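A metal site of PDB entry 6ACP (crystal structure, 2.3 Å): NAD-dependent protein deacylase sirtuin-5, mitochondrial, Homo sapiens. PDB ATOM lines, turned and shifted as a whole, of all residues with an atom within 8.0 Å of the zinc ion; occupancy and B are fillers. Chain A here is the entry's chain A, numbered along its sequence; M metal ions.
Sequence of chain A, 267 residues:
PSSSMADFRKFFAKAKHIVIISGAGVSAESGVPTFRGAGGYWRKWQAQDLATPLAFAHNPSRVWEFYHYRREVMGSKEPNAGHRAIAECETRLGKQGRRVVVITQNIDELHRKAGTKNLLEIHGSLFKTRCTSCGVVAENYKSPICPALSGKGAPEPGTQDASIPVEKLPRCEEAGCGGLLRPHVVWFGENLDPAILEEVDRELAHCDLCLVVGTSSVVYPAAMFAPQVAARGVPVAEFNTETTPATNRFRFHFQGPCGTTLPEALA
SG of Cys 134 lies close to N of Val 136 (3.7 Å). O of Val 136 is in hydrogen-bond range of N of Cys 131 (3.2 Å). SG of Cys 131 sits close to N of Ser 133, 3.3 Å away. N of Glu 174 lies close to SG of Cys 172, 3.5 Å away. N of Cys 172 is in hydrogen-bond range of O of Gly 179 (2.6 Å). SG of Cys 177 sits close to N of Gly 179, 3.4 Å away.
Of the 19 residues printed, 4 come within 4 Å of the zinc ion. The nearest printed residue that does not touch the zinc ion is Val 136 (4.4 Å).
The side-chain sulfur (SG) of Cys 134 binds the zinc ion. SG of Cys 131 is bound to the zinc ion. SG of Cys 172 binds the zinc ion (2.3 Å). SG of Cys 177 is bound to the zinc ion (2.3 Å).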
ATOM      1  N   ARG A 130     -21.227  11.914   5.395  1.00  0.00           N
ATOM      2  CA  ARG A 130     -20.879  13.200   5.946  1.00  0.00           C
ATOM      3  C   ARG A 130     -19.423  13.148   6.345  1.00  0.00           C
ATOM      4  O   ARG A 130     -19.040  12.227   7.002  1.00  0.00           O
ATOM      5  CB  ARG A 130     -21.753  13.580   7.142  1.00  0.00           C
ATOM      6  CG  ARG A 130     -21.480  15.006   7.633  1.00  0.00           C
ATOM      7  CD  ARG A 130     -22.448  15.556   8.636  1.00  0.00           C
ATOM      8  NE  ARG A 130     -22.295  14.940   9.926  1.00  0.00           N
ATOM      9  CZ  ARG A 130     -23.225  14.237  10.589  1.00  0.00           C
ATOM     10  NH1 ARG A 130     -24.424  13.998  10.095  1.00  0.00           N
ATOM     11  NH2 ARG A 130     -22.951  13.760  11.796  1.00  0.00           N
ATOM     12  N   CYS A 131     -18.623  14.131   5.933  1.00  0.00           N
ATOM     13  CA  CYS A 131     -17.194  14.150   6.247  1.00  0.00           C
ATOM     14  C   CYS A 131     -17.014  14.643   7.656  1.00  0.00           C
ATOM     15  O   CYS A 131     -17.617  15.635   8.038  1.00  0.00           O
ATOM     16  CB  CYS A 131     -16.465  15.074   5.305  1.00  0.00           C
ATOM     17  SG  CYS A 131     -14.690  15.270   5.626  1.00  0.00           S
ATOM     18  N   THR A 132     -16.271  13.902   8.449  1.00  0.00           N
ATOM     19  CA  THR A 132     -16.034  14.281   9.830  1.00  0.00           C
ATOM     20  C   THR A 132     -14.908  15.337   9.970  1.00  0.00           C
ATOM     21  O   THR A 132     -14.606  15.701  11.095  1.00  0.00           O
ATOM     22  CB  THR A 132     -15.679  13.043  10.689  1.00  0.00           C
ATOM     23  OG1 THR A 132     -14.456  12.505  10.245  1.00  0.00           O
ATOM     24  CG2 THR A 132     -16.738  11.962  10.603  1.00  0.00           C
ATOM     25  N   SER A 133     -14.269  15.745   8.871  1.00  0.00           N
ATOM     26  CA  SER A 133     -13.304  16.848   8.873  1.00  0.00           C
ATOM     27  C   SER A 133     -14.009  18.132   8.476  1.00  0.00           C
ATOM     28  O   SER A 133     -14.158  19.017   9.315  1.00  0.00           O
ATOM     29  CB  SER A 133     -12.128  16.585   7.939  1.00  0.00           C
ATOM     30  OG  SER A 133     -11.344  15.525   8.445  1.00  0.00           O
ATOM     31  N   CYS A 134     -14.519  18.199   7.232  1.00  0.00           N
ATOM     32  CA  CYS A 134     -15.212  19.422   6.709  1.00  0.00           C
ATOM     33  C   CYS A 134     -16.759  19.481   6.809  1.00  0.00           C
ATOM     34  O   CYS A 134     -17.358  20.502   6.460  1.00  0.00           O
ATOM     35  CB  CYS A 134     -14.788  19.627   5.264  1.00  0.00           C
ATOM     36  SG  CYS A 134     -15.503  18.536   4.011  1.00  0.00           S
ATOM     37  N   GLY A 135     -17.434  18.423   7.231  1.00  0.00           N
ATOM     38  CA  GLY A 135     -18.899  18.485   7.350  1.00  0.00           C
ATOM     39  C   GLY A 135     -19.718  18.522   6.057  1.00  0.00           C
ATOM     40  O   GLY A 135     -20.920  18.640   6.116  1.00  0.00           O
ATOM     41  N   VAL A 136     -19.115  18.454   4.881  1.00  0.00           N
ATOM     42  CA  VAL A 136     -19.956  18.412   3.687  1.00  0.00           C
ATOM     43  C   VAL A 136     -20.784  17.103   3.686  1.00  0.00           C
ATOM     44  O   VAL A 136     -20.270  16.027   3.984  1.00  0.00           O
ATOM     45  CB  VAL A 136     -19.142  18.560   2.383  1.00  0.00           C
ATOM     46  CG1 VAL A 136     -18.194  17.388   2.194  1.00  0.00           C
ATOM     47  CG2 VAL A 136     -20.080  18.707   1.184  1.00  0.00           C
ATOM     48  N   VAL A 137     -22.072  17.254   3.449  1.00  0.00           N
ATOM     49  CA  VAL A 137     -23.003  16.140   3.266  1.00  0.00           C
ATOM     50  C   VAL A 137     -23.105  15.867   1.793  1.00  0.00           C
ATOM     51  O   VAL A 137     -23.480  16.760   1.061  1.00  0.00           O
ATOM     52  CB  VAL A 137     -24.405  16.569   3.737  1.00  0.00           C
ATOM     53  CG1 VAL A 137     -25.417  15.481   3.435  1.00  0.00           C
ATOM     54  CG2 VAL A 137     -24.373  16.960   5.235  1.00  0.00           C
ATOM     55  N   ARG A 171     -13.043   8.147   2.310  1.00  0.00           N
ATOM     56  CA  ARG A 171     -12.451   9.443   2.548  1.00  0.00           C
ATOM     57  C   ARG A 171     -13.170  10.490   1.731  1.00  0.00           C
ATOM     58  O   ARG A 171     -13.654  10.241   0.624  1.00  0.00           O
ATOM     59  CB  ARG A 171     -10.987   9.429   2.147  1.00  0.00           C
ATOM     60  CG  ARG A 171     -10.136   8.346   2.771  1.00  0.00           C
ATOM     61  CD  ARG A 171     -10.219   8.268   4.310  1.00  0.00           C
ATOM     62  NE  ARG A 171      -9.593   9.423   5.001  1.00  0.00           N
ATOM     63  CZ  ARG A 171      -9.154   9.398   6.261  1.00  0.00           C
ATOM     64  NH1 ARG A 171      -9.254   8.312   7.027  1.00  0.00           N
ATOM     65  NH2 ARG A 171      -8.655  10.486   6.786  1.00  0.00           N
ATOM     66  N   CYS A 172     -13.224  11.680   2.284  1.00  0.00           N
ATOM     67  CA  CYS A 172     -13.816  12.835   1.615  1.00  0.00           C
ATOM     68  C   CYS A 172     -13.158  13.066   0.276  1.00  0.00           C
ATOM     69  O   CYS A 172     -11.939  12.969   0.186  1.00  0.00           O
ATOM     70  CB  CYS A 172     -13.587  14.073   2.460  1.00  0.00           C
ATOM     71  SG  CYS A 172     -14.413  15.528   1.849  1.00  0.00           S
ATOM     72  N   GLU A 173     -13.924  13.370  -0.774  1.00  0.00           N
ATOM     73  CA  GLU A 173     -13.311  13.641  -2.075  1.00  0.00           C
ATOM     74  C   GLU A 173     -13.110  15.130  -2.396  1.00  0.00           C
ATOM     75  O   GLU A 173     -12.404  15.450  -3.360  1.00  0.00           O
ATOM     76  CB  GLU A 173     -14.040  12.892  -3.192  1.00  0.00           C
ATOM     77  CG  GLU A 173     -13.964  11.370  -3.013  1.00  0.00           C
ATOM     78  CD  GLU A 173     -13.563  10.598  -4.274  1.00  0.00           C
ATOM     79  OE1 GLU A 173     -13.877  11.021  -5.413  1.00  0.00           O
ATOM     80  OE2 GLU A 173     -12.926   9.522  -4.130  1.00  0.00           O
ATOM     81  N   GLU A 174     -13.679  16.019  -1.587  1.00  0.00           N
ATOM     82  CA  GLU A 174     -13.406  17.451  -1.677  1.00  0.00           C
ATOM     83  C   GLU A 174     -11.898  17.732  -1.815  1.00  0.00           C
ATOM     84  O   GLU A 174     -11.065  17.146  -1.112  1.00  0.00           O
ATOM     85  CB  GLU A 174     -13.920  18.159  -0.453  1.00  0.00           C
ATOM     86  CG  GLU A 174     -15.417  18.205  -0.304  1.00  0.00           C
ATOM     87  CD  GLU A 174     -16.080  19.075  -1.350  1.00  0.00           C
ATOM     88  OE1 GLU A 174     -15.755  20.294  -1.435  1.00  0.00           O
ATOM     89  OE2 GLU A 174     -16.935  18.538  -2.067  1.00  0.00           O
ATOM     90  N   ALA A 175     -11.533  18.561  -2.777  1.00  0.00           N
ATOM     91  CA  ALA A 175     -10.123  18.900  -2.994  1.00  0.00           C
ATOM     92  C   ALA A 175      -9.493  19.408  -1.695  1.00  0.00           C
ATOM     93  O   ALA A 175      -9.987  20.368  -1.070  1.00  0.00           O
ATOM     94  CB  ALA A 175     -10.017  19.949  -4.082  1.00  0.00           C
ATOM     95  N   GLY A 176      -8.461  18.713  -1.241  1.00  0.00           N
ATOM     96  CA  GLY A 176      -7.662  19.168  -0.106  1.00  0.00           C
ATOM     97  C   GLY A 176      -8.041  18.621   1.247  1.00  0.00           C
ATOM     98  O   GLY A 176      -7.298  18.850   2.208  1.00  0.00           O
ATOM     99  N   CYS A 177      -9.136  17.872   1.333  1.00  0.00           N
ATOM    100  CA  CYS A 177      -9.662  17.473   2.623  1.00  0.00           C
ATOM    101  C   CYS A 177      -9.063  16.157   3.133  1.00  0.00           C
ATOM    102  O   CYS A 177      -8.402  16.124   4.209  1.00  0.00           O
ATOM    103  CB  CYS A 177     -11.205  17.415   2.588  1.00  0.00           C
ATOM    104  SG  CYS A 177     -11.894  16.981   4.201  1.00  0.00           S
ATOM    105  N   GLY A 178      -9.354  15.065   2.421  1.00  0.00           N
ATOM    106  CA  GLY A 178      -8.935  13.726   2.878  1.00  0.00           C
ATOM    107  C   GLY A 178      -9.613  13.218   4.162  1.00  0.00           C
ATOM    108  O   GLY A 178      -9.223  12.172   4.688  1.00  0.00           O
ATOM    109  N   GLY A 179     -10.633  13.897   4.653  1.00  0.00           N
ATOM    110  CA  GLY A 179     -11.261  13.548   5.933  1.00  0.00           C
ATOM    111  C   GLY A 179     -11.982  12.215   5.854  1.00  0.00           C
ATOM    112  O   GLY A 179     -12.302  11.756   4.759  1.00  0.00           O
ATOM    113  N   LEU A 180     -12.152  11.582   7.002  1.00  0.00           N
ATOM    114  CA  LEU A 180     -12.822  10.300   7.118  1.00  0.00           C
ATOM    115  C   LEU A 180     -14.324  10.536   7.010  1.00  0.00           C
ATOM    116  O   LEU A 180     -14.876  11.348   7.732  1.00  0.00           O
ATOM    117  CB  LEU A 180     -12.486   9.645   8.456  1.00  0.00           C
ATOM    118  CG  LEU A 180     -13.399   8.484   8.849  1.00  0.00           C
ATOM    119  CD1 LEU A 180     -13.343   7.277   7.889  1.00  0.00           C
ATOM    120  CD2 LEU A 180     -13.029   8.085  10.261  1.00  0.00           C
ATOM    121  N   LEU A 181     -14.993   9.824   6.105  1.00  0.00           N
ATOM    122  CA  LEU A 181     -16.433   9.942   6.036  1.00  0.00           C
ATOM    123  C   LEU A 181     -17.107   9.061   7.069  1.00  0.00           C
ATOM    124  O   LEU A 181     -16.588   8.016   7.407  1.00  0.00           O
ATOM    125  CB  LEU A 181     -16.960   9.594   4.612  1.00  0.00           C
ATOM    126  CG  LEU A 181     -16.448  10.473   3.495  1.00  0.00           C
ATOM    127  CD1 LEU A 181     -16.803   9.965   2.074  1.00  0.00           C
ATOM    128  CD2 LEU A 181     -16.938  11.903   3.654  1.00  0.00           C
HETATM  129 ZN    ZN M   1     -14.188  16.691   3.860  1.00  0.00          ZN
